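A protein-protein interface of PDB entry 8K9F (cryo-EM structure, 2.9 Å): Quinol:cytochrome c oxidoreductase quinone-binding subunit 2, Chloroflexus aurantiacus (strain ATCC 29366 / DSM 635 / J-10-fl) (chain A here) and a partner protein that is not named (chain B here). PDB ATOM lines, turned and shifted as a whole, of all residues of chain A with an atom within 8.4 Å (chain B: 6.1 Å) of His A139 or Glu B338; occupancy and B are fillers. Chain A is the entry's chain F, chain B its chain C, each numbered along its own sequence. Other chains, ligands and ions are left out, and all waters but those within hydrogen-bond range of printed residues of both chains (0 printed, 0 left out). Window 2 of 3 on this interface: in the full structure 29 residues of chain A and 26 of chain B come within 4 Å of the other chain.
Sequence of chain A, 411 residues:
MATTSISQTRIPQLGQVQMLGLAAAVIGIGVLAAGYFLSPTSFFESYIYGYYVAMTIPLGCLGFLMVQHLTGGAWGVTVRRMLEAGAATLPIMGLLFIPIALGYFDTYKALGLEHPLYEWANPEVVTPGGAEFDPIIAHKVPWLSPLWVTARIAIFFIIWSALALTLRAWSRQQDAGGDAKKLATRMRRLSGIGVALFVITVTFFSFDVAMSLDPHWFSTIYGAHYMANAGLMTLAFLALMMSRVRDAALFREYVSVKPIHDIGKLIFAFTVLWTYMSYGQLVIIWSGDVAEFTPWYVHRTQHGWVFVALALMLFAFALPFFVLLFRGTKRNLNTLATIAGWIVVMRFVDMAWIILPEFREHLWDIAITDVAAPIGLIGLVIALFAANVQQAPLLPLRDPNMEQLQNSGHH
OE2 of Glu B338 lies within hydrogen-bond range of NE2 of His A139 (3.1 Å). The backbone carbonyl oxygen of Ser B332 lies close to a ring nitrogen (ND1) of His A139 (3.5 Å). The backbone carbonyl oxygen (O) of Tyr B331 is in hydrogen-bond range of the side-chain amino group (NZ) of Lys A140 (3.3 Å).
The side-chain hydroxyl (OG) of Ser B332 sits at hydrogen-bond distance from the backbone NH (N) of Asn B334 (2.8 Å). O of Ile A136 is in hydrogen-bond range of NZ of Lys A140, at 2.4 Å.
Among the printed residues, merely in contact across the chains: His A139 with Leu B330 (3.2 Å), His A139 with Tyr B331 (3.99 Å), His A139 with Gly B333 (3.8 Å) and Leu A144 with Tyr B331 (3.8 Å).
Glu B338 touches just one residue of chain A: His A139 (3.1 Å). Of the printed residues of chain B, Lys A140 touches Tyr B331. Printed residues of chain B within 4 Å of Leu A144: Tyr B331 (3.8 Å). The nearest printed residue of chain B that does not touch Lys A140 is Gly B333 (4.5 Å).
Of the 15 printed residues of chain B, 5 touch a printed residue of chain A. Hydrophobic or aromatic side chains of chain B within 4 Å of the printed part of chain A: Tyr B331. Printed residues of chain A that touch a printed residue of chain B: His A139, Lys A140 and Leu A144. Hydrophobic or aromatic side chains of chain A that line the printed part of chain B: His A139 and Leu A144. Among the printed residues, no Asp or Glu carboxylate lies within 4 Å of a Lys or Arg side-chain nitrogen of the other chain.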
ATOM      1  N   VAL A 125     -31.212 -19.386  -8.873  1.00  0.00           N
ATOM      2  CA  VAL A 125     -31.309 -18.342  -9.884  1.00  0.00           C
ATOM      3  C   VAL A 125     -30.210 -18.476 -10.936  1.00  0.00           C
ATOM      4  O   VAL A 125     -30.337 -17.913 -12.030  1.00  0.00           O
ATOM      5  CB  VAL A 125     -31.326 -16.975  -9.170  1.00  0.00           C
ATOM      6  CG1 VAL A 125     -31.833 -15.862 -10.072  1.00  0.00           C
ATOM      7  CG2 VAL A 125     -32.228 -17.050  -7.957  1.00  0.00           C
ATOM      8  N   VAL A 126     -29.154 -19.240 -10.664  1.00  0.00           N
ATOM      9  CA  VAL A 126     -28.074 -19.404 -11.629  1.00  0.00           C
ATOM     10  C   VAL A 126     -27.856 -20.846 -12.067  1.00  0.00           C
ATOM     11  O   VAL A 126     -27.121 -21.065 -13.045  1.00  0.00           O
ATOM     12  CB  VAL A 126     -26.747 -18.819 -11.100  1.00  0.00           C
ATOM     13  CG1 VAL A 126     -26.886 -17.345 -10.775  1.00  0.00           C
ATOM     14  CG2 VAL A 126     -26.268 -19.594  -9.896  1.00  0.00           C
ATOM     15  N   PHE A 133     -33.887 -20.490 -12.844  1.00  0.00           N
ATOM     16  CA  PHE A 133     -33.161 -20.362 -14.114  1.00  0.00           C
ATOM     17  C   PHE A 133     -33.415 -19.010 -14.779  1.00  0.00           C
ATOM     18  O   PHE A 133     -33.795 -18.932 -15.947  1.00  0.00           O
ATOM     19  CB  PHE A 133     -33.511 -21.506 -15.075  1.00  0.00           C
ATOM     20  CG  PHE A 133     -32.855 -21.402 -16.431  1.00  0.00           C
ATOM     21  CD1 PHE A 133     -31.533 -21.790 -16.630  1.00  0.00           C
ATOM     22  CD2 PHE A 133     -33.561 -20.878 -17.505  1.00  0.00           C
ATOM     23  CE1 PHE A 133     -30.936 -21.676 -17.874  1.00  0.00           C
ATOM     24  CE2 PHE A 133     -32.969 -20.761 -18.756  1.00  0.00           C
ATOM     25  CZ  PHE A 133     -31.653 -21.160 -18.936  1.00  0.00           C
ATOM     26  N   ASP A 134     -33.218 -17.945 -14.013  1.00  0.00           N
ATOM     27  CA  ASP A 134     -33.366 -16.609 -14.574  1.00  0.00           C
ATOM     28  C   ASP A 134     -32.186 -16.355 -15.499  1.00  0.00           C
ATOM     29  O   ASP A 134     -31.047 -16.293 -15.024  1.00  0.00           O
ATOM     30  CB  ASP A 134     -33.431 -15.566 -13.468  1.00  0.00           C
ATOM     31  CG  ASP A 134     -33.540 -14.151 -14.001  1.00  0.00           C
ATOM     32  OD1 ASP A 134     -34.143 -13.950 -15.074  1.00  0.00           O
ATOM     33  OD2 ASP A 134     -33.038 -13.229 -13.338  1.00  0.00           O
ATOM     34  N   PRO A 135     -32.402 -16.209 -16.812  1.00  0.00           N
ATOM     35  CA  PRO A 135     -31.275 -16.283 -17.749  1.00  0.00           C
ATOM     36  C   PRO A 135     -30.396 -15.050 -17.778  1.00  0.00           C
ATOM     37  O   PRO A 135     -29.277 -15.141 -18.295  1.00  0.00           O
ATOM     38  CB  PRO A 135     -31.962 -16.493 -19.107  1.00  0.00           C
ATOM     39  CG  PRO A 135     -33.389 -16.833 -18.782  1.00  0.00           C
ATOM     40  CD  PRO A 135     -33.677 -16.092 -17.529  1.00  0.00           C
ATOM     41  N   ILE A 136     -30.861 -13.904 -17.277  1.00  0.00           N
ATOM     42  CA  ILE A 136     -29.989 -12.736 -17.201  1.00  0.00           C
ATOM     43  C   ILE A 136     -28.926 -12.936 -16.132  1.00  0.00           C
ATOM     44  O   ILE A 136     -27.744 -12.647 -16.349  1.00  0.00           O
ATOM     45  CB  ILE A 136     -30.814 -11.462 -16.953  1.00  0.00           C
ATOM     46  CG1 ILE A 136     -31.919 -11.332 -18.002  1.00  0.00           C
ATOM     47  CG2 ILE A 136     -29.923 -10.230 -16.963  1.00  0.00           C
ATOM     48  CD1 ILE A 136     -31.405 -11.247 -19.416  1.00  0.00           C
ATOM     49  N   ILE A 137     -29.320 -13.455 -14.969  1.00  0.00           N
ATOM     50  CA  ILE A 137     -28.360 -13.711 -13.904  1.00  0.00           C
ATOM     51  C   ILE A 137     -27.566 -14.978 -14.187  1.00  0.00           C
ATOM     52  O   ILE A 137     -26.389 -15.073 -13.821  1.00  0.00           O
ATOM     53  CB  ILE A 137     -29.098 -13.762 -12.558  1.00  0.00           C
ATOM     54  CG1 ILE A 137     -29.988 -12.527 -12.440  1.00  0.00           C
ATOM     55  CG2 ILE A 137     -28.129 -13.815 -11.389  1.00  0.00           C
ATOM     56  CD1 ILE A 137     -30.702 -12.390 -11.133  1.00  0.00           C
ATOM     57  N   ALA A 138     -28.164 -15.950 -14.872  1.00  0.00           N
ATOM     58  CA  ALA A 138     -27.447 -17.165 -15.230  1.00  0.00           C
ATOM     59  C   ALA A 138     -26.484 -16.969 -16.390  1.00  0.00           C
ATOM     60  O   ALA A 138     -25.638 -17.835 -16.624  1.00  0.00           O
ATOM     61  CB  ALA A 138     -28.430 -18.281 -15.576  1.00  0.00           C
ATOM     62  N   HIS A 139     -26.610 -15.879 -17.147  1.00  0.00           N
ATOM     63  CA  HIS A 139     -25.650 -15.621 -18.215  1.00  0.00           C
ATOM     64  C   HIS A 139     -24.302 -15.193 -17.650  1.00  0.00           C
ATOM     65  O   HIS A 139     -23.250 -15.596 -18.158  1.00  0.00           O
ATOM     66  CB  HIS A 139     -26.191 -14.555 -19.164  1.00  0.00           C
ATOM     67  CG  HIS A 139     -25.210 -14.122 -20.206  1.00  0.00           C
ATOM     68  ND1 HIS A 139     -24.611 -12.883 -20.195  1.00  0.00           N
ATOM     69  CD2 HIS A 139     -24.711 -14.774 -21.283  1.00  0.00           C
ATOM     70  CE1 HIS A 139     -23.792 -12.784 -21.225  1.00  0.00           C
ATOM     71  NE2 HIS A 139     -23.832 -13.919 -21.901  1.00  0.00           N
ATOM     72  N   LYS A 140     -24.319 -14.384 -16.593  1.00  0.00           N
ATOM     73  CA  LYS A 140     -23.122 -13.820 -15.988  1.00  0.00           C
ATOM     74  C   LYS A 140     -22.569 -14.679 -14.855  1.00  0.00           C
ATOM     75  O   LYS A 140     -21.917 -14.145 -13.951  1.00  0.00           O
ATOM     76  CB  LYS A 140     -23.425 -12.411 -15.479  1.00  0.00           C
ATOM     77  CG  LYS A 140     -24.669 -12.347 -14.619  1.00  0.00           C
ATOM     78  CD  LYS A 140     -25.000 -10.938 -14.169  1.00  0.00           C
ATOM     79  CE  LYS A 140     -25.397 -10.037 -15.310  1.00  0.00           C
ATOM     80  NZ  LYS A 140     -26.366 -10.679 -16.225  1.00  0.00           N
ATOM     81  N   VAL A 141     -22.838 -15.981 -14.858  1.00  0.00           N
ATOM     82  CA  VAL A 141     -22.398 -16.882 -13.789  1.00  0.00           C
ATOM     83  C   VAL A 141     -20.879 -17.134 -13.747  1.00  0.00           C
ATOM     84  O   VAL A 141     -20.383 -17.415 -12.642  1.00  0.00           O
ATOM     85  CB  VAL A 141     -23.222 -18.198 -13.815  1.00  0.00           C
ATOM     86  CG1 VAL A 141     -23.047 -19.032 -15.080  1.00  0.00           C
ATOM     87  CG2 VAL A 141     -23.090 -19.036 -12.530  1.00  0.00           C
ATOM     88  N   PRO A 142     -20.056 -17.039 -14.818  1.00  0.00           N
ATOM     89  CA  PRO A 142     -18.609 -17.059 -14.522  1.00  0.00           C
ATOM     90  C   PRO A 142     -18.139 -15.795 -13.830  1.00  0.00           C
ATOM     91  O   PRO A 142     -17.306 -15.872 -12.920  1.00  0.00           O
ATOM     92  CB  PRO A 142     -17.930 -17.230 -15.886  1.00  0.00           C
ATOM     93  CG  PRO A 142     -18.947 -17.261 -16.876  1.00  0.00           C
ATOM     94  CD  PRO A 142     -20.282 -17.139 -16.281  1.00  0.00           C
ATOM     95  N   TRP A 143     -18.670 -14.635 -14.216  1.00  0.00           N
ATOM     96  CA  TRP A 143     -18.211 -13.392 -13.612  1.00  0.00           C
ATOM     97  C   TRP A 143     -18.775 -13.214 -12.212  1.00  0.00           C
ATOM     98  O   TRP A 143     -18.087 -12.711 -11.319  1.00  0.00           O
ATOM     99  CB  TRP A 143     -18.607 -12.201 -14.477  1.00  0.00           C
ATOM    100  CG  TRP A 143     -17.864 -10.929 -14.171  1.00  0.00           C
ATOM    101  CD1 TRP A 143     -18.420  -9.713 -13.960  1.00  0.00           C
ATOM    102  CD2 TRP A 143     -16.439 -10.717 -14.188  1.00  0.00           C
ATOM    103  NE1 TRP A 143     -17.447  -8.772 -13.752  1.00  0.00           N
ATOM    104  CE2 TRP A 143     -16.221  -9.358 -13.903  1.00  0.00           C
ATOM    105  CE3 TRP A 143     -15.329 -11.547 -14.387  1.00  0.00           C
ATOM    106  CZ2 TRP A 143     -14.948  -8.809 -13.813  1.00  0.00           C
ATOM    107  CZ3 TRP A 143     -14.067 -11.001 -14.289  1.00  0.00           C
ATOM    108  CH2 TRP A 143     -13.888  -9.642 -14.009  1.00  0.00           C
ATOM    109  N   LEU A 144     -20.027 -13.598 -12.005  1.00  0.00           N
ATOM    110  CA  LEU A 144     -20.700 -13.407 -10.726  1.00  0.00           C
ATOM    111  C   LEU A 144     -20.987 -14.785 -10.146  1.00  0.00           C
ATOM    112  O   LEU A 144     -22.068 -15.347 -10.316  1.00  0.00           O
ATOM    113  CB  LEU A 144     -21.959 -12.577 -10.887  1.00  0.00           C
ATOM    114  CG  LEU A 144     -21.728 -11.104 -11.229  1.00  0.00           C
ATOM    115  CD1 LEU A 144     -23.016 -10.321 -11.131  1.00  0.00           C
ATOM    116  CD2 LEU A 144     -20.678 -10.483 -10.336  1.00  0.00           C
ATOM    117  N   SER B 329     -21.062  -4.943 -22.865  1.00  0.00           N
ATOM    118  CA  SER B 329     -21.487  -5.905 -23.868  1.00  0.00           C
ATOM    119  C   SER B 329     -21.375  -7.342 -23.367  1.00  0.00           C
ATOM    120  O   SER B 329     -22.179  -8.195 -23.754  1.00  0.00           O
ATOM    121  CB  SER B 329     -20.675  -5.698 -25.136  1.00  0.00           C
ATOM    122  OG  SER B 329     -21.008  -4.462 -25.742  1.00  0.00           O
ATOM    123  N   LEU B 330     -20.396  -7.631 -22.508  1.00  0.00           N
ATOM    124  CA  LEU B 330     -20.228  -8.998 -22.021  1.00  0.00           C
ATOM    125  C   LEU B 330     -21.121  -9.295 -20.824  1.00  0.00           C
ATOM    126  O   LEU B 330     -21.703 -10.380 -20.739  1.00  0.00           O
ATOM    127  CB  LEU B 330     -18.767  -9.249 -21.658  1.00  0.00           C
ATOM    128  CG  LEU B 330     -17.838  -9.594 -22.819  1.00  0.00           C
ATOM    129  CD1 LEU B 330     -16.509 -10.088 -22.291  1.00  0.00           C
ATOM    130  CD2 LEU B 330     -18.473 -10.638 -23.724  1.00  0.00           C
ATOM    131  N   TYR B 331     -21.228  -8.347 -19.896  1.00  0.00           N
ATOM    132  CA  TYR B 331     -21.999  -8.531 -18.674  1.00  0.00           C
ATOM    133  C   TYR B 331     -23.490  -8.634 -18.959  1.00  0.00           C
ATOM    134  O   TYR B 331     -24.193  -9.401 -18.296  1.00  0.00           O
ATOM    135  CB  TYR B 331     -21.692  -7.369 -17.729  1.00  0.00           C
ATOM    136  CG  TYR B 331     -22.440  -7.318 -16.418  1.00  0.00           C
ATOM    137  CD1 TYR B 331     -21.984  -8.015 -15.307  1.00  0.00           C
ATOM    138  CD2 TYR B 331     -23.574  -6.526 -16.277  1.00  0.00           C
ATOM    139  CE1 TYR B 331     -22.653  -7.949 -14.102  1.00  0.00           C
ATOM    140  CE2 TYR B 331     -24.251  -6.458 -15.080  1.00  0.00           C
ATOM    141  CZ  TYR B 331     -23.786  -7.170 -13.994  1.00  0.00           C
ATOM    142  OH  TYR B 331     -24.462  -7.097 -12.799  1.00  0.00           O
ATOM    143  N   SER B 332     -23.983  -7.884 -19.939  1.00  0.00           N
ATOM    144  CA  SER B 332     -25.403  -7.894 -20.267  1.00  0.00           C
ATOM    145  C   SER B 332     -25.821  -9.204 -20.917  1.00  0.00           C
ATOM    146  O   SER B 332     -25.092  -9.780 -21.725  1.00  0.00           O
ATOM    147  CB  SER B 332     -25.730  -6.748 -21.211  1.00  0.00           C
ATOM    148  OG  SER B 332     -26.905  -6.999 -21.954  1.00  0.00           O
ATOM    149  N   GLY B 333     -27.014  -9.663 -20.570  1.00  0.00           N
ATOM    150  CA  GLY B 333     -27.610 -10.803 -21.225  1.00  0.00           C
ATOM    151  C   GLY B 333     -28.381 -10.472 -22.476  1.00  0.00           C
ATOM    152  O   GLY B 333     -28.988 -11.365 -23.071  1.00  0.00           O
ATOM    153  N   ASN B 334     -28.391  -9.206 -22.886  1.00  0.00           N
ATOM    154  CA  ASN B 334     -29.102  -8.813 -24.091  1.00  0.00           C
ATOM    155  C   ASN B 334     -28.349  -9.286 -25.321  1.00  0.00           C
ATOM    156  O   ASN B 334     -27.118  -9.322 -25.336  1.00  0.00           O
ATOM    157  CB  ASN B 334     -29.285  -7.298 -24.141  1.00  0.00           C
ATOM    158  CG  ASN B 334     -30.698  -6.895 -24.475  1.00  0.00           C
ATOM    159  OD1 ASN B 334     -31.638  -7.665 -24.277  1.00  0.00           O
ATOM    160  ND2 ASN B 334     -30.861  -5.682 -24.986  1.00  0.00           N
ATOM    161  N   GLU B 335     -29.102  -9.665 -26.352  1.00  0.00           N
ATOM    162  CA  GLU B 335     -28.485 -10.080 -27.604  1.00  0.00           C
ATOM    163  C   GLU B 335     -27.838  -8.901 -28.318  1.00  0.00           C
ATOM    164  O   GLU B 335     -26.812  -9.068 -28.985  1.00  0.00           O
ATOM    165  CB  GLU B 335     -29.543 -10.769 -28.482  1.00  0.00           C
ATOM    166  CG  GLU B 335     -29.584 -10.416 -29.976  1.00  0.00           C
ATOM    167  CD  GLU B 335     -28.436 -11.009 -30.792  1.00  0.00           C
ATOM    168  OE1 GLU B 335     -27.634 -11.797 -30.244  1.00  0.00           O
ATOM    169  OE2 GLU B 335     -28.328 -10.671 -31.989  1.00  0.00           O
ATOM    170  N   PHE B 336     -28.389  -7.701 -28.143  1.00  0.00           N
ATOM    171  CA  PHE B 336     -28.026  -6.572 -28.992  1.00  0.00           C
ATOM    172  C   PHE B 336     -26.670  -5.990 -28.610  1.00  0.00           C
ATOM    173  O   PHE B 336     -25.876  -5.638 -29.489  1.00  0.00           O
ATOM    174  CB  PHE B 336     -29.140  -5.523 -28.939  1.00  0.00           C
ATOM    175  CG  PHE B 336     -30.477  -6.057 -29.388  1.00  0.00           C
ATOM    176  CD1 PHE B 336     -31.346  -6.661 -28.486  1.00  0.00           C
ATOM    177  CD2 PHE B 336     -30.847  -5.991 -30.718  1.00  0.00           C
ATOM    178  CE1 PHE B 336     -32.538  -7.192 -28.905  1.00  0.00           C
ATOM    179  CE2 PHE B 336     -32.062  -6.504 -31.135  1.00  0.00           C
ATOM    180  CZ  PHE B 336     -32.905  -7.101 -30.227  1.00  0.00           C
ATOM    181  N   GLU B 337     -26.365  -5.930 -27.309  1.00  0.00           N
ATOM    182  CA  GLU B 337     -25.038  -5.505 -26.867  1.00  0.00           C
ATOM    183  C   GLU B 337     -23.969  -6.533 -27.235  1.00  0.00           C
ATOM    184  O   GLU B 337     -22.838  -6.172 -27.589  1.00  0.00           O
ATOM    185  CB  GLU B 337     -25.046  -5.263 -25.359  1.00  0.00           C
ATOM    186  CG  GLU B 337     -26.007  -4.179 -24.896  1.00  0.00           C
ATOM    187  CD  GLU B 337     -25.295  -2.907 -24.472  1.00  0.00           C
ATOM    188  OE1 GLU B 337     -25.976  -1.958 -24.031  1.00  0.00           O
ATOM    189  OE2 GLU B 337     -24.054  -2.852 -24.581  1.00  0.00           O
ATOM    190  N   GLU B 338     -24.310  -7.819 -27.157  1.00  0.00           N
ATOM    191  CA  GLU B 338     -23.366  -8.857 -27.550  1.00  0.00           C
ATOM    192  C   GLU B 338     -23.083  -8.821 -29.045  1.00  0.00           C
ATOM    193  O   GLU B 338     -21.933  -8.980 -29.467  1.00  0.00           O
ATOM    194  CB  GLU B 338     -23.892 -10.227 -27.142  1.00  0.00           C
ATOM    195  CG  GLU B 338     -24.010 -10.414 -25.648  1.00  0.00           C
ATOM    196  CD  GLU B 338     -24.633 -11.736 -25.300  1.00  0.00           C
ATOM    197  OE1 GLU B 338     -24.935 -12.504 -26.237  1.00  0.00           O
ATOM    198  OE2 GLU B 338     -24.827 -12.010 -24.098  1.00  0.00           O
ATOM    199  N   TYR B 339     -24.112  -8.598 -29.863  1.00  0.00           N
ATOM    200  CA  TYR B 339     -23.868  -8.509 -31.296  1.00  0.00           C
ATOM    201  C   TYR B 339     -23.170  -7.210 -31.658  1.00  0.00           C
ATOM    202  O   TYR B 339     -22.453  -7.164 -32.659  1.00  0.00           O
ATOM    203  CB  TYR B 339     -25.158  -8.648 -32.093  1.00  0.00           C
ATOM    204  CG  TYR B 339     -24.887  -9.033 -33.527  1.00  0.00           C
ATOM    205  CD1 TYR B 339     -24.679 -10.357 -33.876  1.00  0.00           C
ATOM    206  CD2 TYR B 339     -24.810  -8.071 -34.523  1.00  0.00           C
ATOM    207  CE1 TYR B 339     -24.415 -10.714 -35.176  1.00  0.00           C
ATOM    208  CE2 TYR B 339     -24.534  -8.414 -35.820  1.00  0.00           C
ATOM    209  CZ  TYR B 339     -24.348  -9.737 -36.147  1.00  0.00           C
ATOM    210  OH  TYR B 339     -24.085 -10.092 -37.449  1.00  0.00           O
ATOM    211  N   LEU B 340     -23.362  -6.160 -30.856  1.00  0.00           N
ATOM    212  CA  LEU B 340     -22.526  -4.969 -30.957  1.00  0.00           C
ATOM    213  C   LEU B 340     -21.053  -5.302 -30.793  1.00  0.00           C
ATOM    214  O   LEU B 340     -20.218  -4.876 -31.600  1.00  0.00           O
ATOM    215  CB  LEU B 340     -22.921  -3.968 -29.889  1.00  0.00           C
ATOM    216  CG  LEU B 340     -22.349  -2.570 -29.978  1.00  0.00           C
ATOM    217  CD1 LEU B 340     -22.931  -1.737 -31.116  1.00  0.00           C
ATOM    218  CD2 LEU B 340     -22.506  -1.970 -28.615  1.00  0.00           C
ATOM    219  N   LEU B 341     -20.716  -6.050 -29.740  1.00  0.00           N
ATOM    220  CA  LEU B 341     -19.313  -6.389 -29.513  1.00  0.00           C
ATOM    221  C   LEU B 341     -18.776  -7.329 -30.582  1.00  0.00           C
ATOM    222  O   LEU B 341     -17.608  -7.221 -30.967  1.00  0.00           O
ATOM    223  CB  LEU B 341     -19.124  -7.011 -28.136  1.00  0.00           C
ATOM    224  CG  LEU B 341     -17.672  -7.095 -27.665  1.00  0.00           C
ATOM    225  CD1 LEU B 341     -17.007  -5.726 -27.727  1.00  0.00           C
ATOM    226  CD2 LEU B 341     -17.598  -7.676 -26.272  1.00  0.00           C
ATOM    227  N   TYR B 342     -19.615  -8.237 -31.083  1.00  0.00           N
ATOM    228  CA  TYR B 342     -19.194  -9.124 -32.163  1.00  0.00           C
ATOM    229  C   TYR B 342     -18.938  -8.349 -33.452  1.00  0.00           C
ATOM    230  O   TYR B 342     -17.886  -8.507 -34.083  1.00  0.00           O
ATOM    231  CB  TYR B 342     -20.249 -10.205 -32.389  1.00  0.00           C
ATOM    232  CG  TYR B 342     -20.020 -11.024 -33.632  1.00  0.00           C
ATOM    233  CD1 TYR B 342     -19.012 -11.978 -33.675  1.00  0.00           C
ATOM    234  CD2 TYR B 342     -20.813 -10.852 -34.763  1.00  0.00           C
ATOM    235  CE1 TYR B 342     -18.791 -12.734 -34.808  1.00  0.00           C
ATOM    236  CE2 TYR B 342     -20.597 -11.603 -35.901  1.00  0.00           C
ATOM    237  CZ  TYR B 342     -19.584 -12.542 -35.916  1.00  0.00           C
ATOM    238  OH  TYR B 342     -19.363 -13.296 -37.043  1.00  0.00           O
ATOM    239  N   ASN B 343     -19.884  -7.497 -33.854  1.00  0.00           N
ATOM    240  CA  ASN B 343     -19.776  -6.743 -35.096  1.00  0.00           C
ATOM    241  C   ASN B 343     -18.701  -5.664 -35.015  1.00  0.00           C
ATOM    242  O   ASN B 343     -18.122  -5.299 -36.042  1.00  0.00           O
ATOM    243  CB  ASN B 343     -21.167  -6.183 -35.436  1.00  0.00           C
ATOM    244  CG  ASN B 343     -21.128  -4.941 -36.289  1.00  0.00           C
ATOM    245  OD1 ASN B 343     -20.763  -4.990 -37.459  1.00  0.00           O
ATOM    246  ND2 ASN B 343     -21.543  -3.822 -35.719  1.00  0.00           N
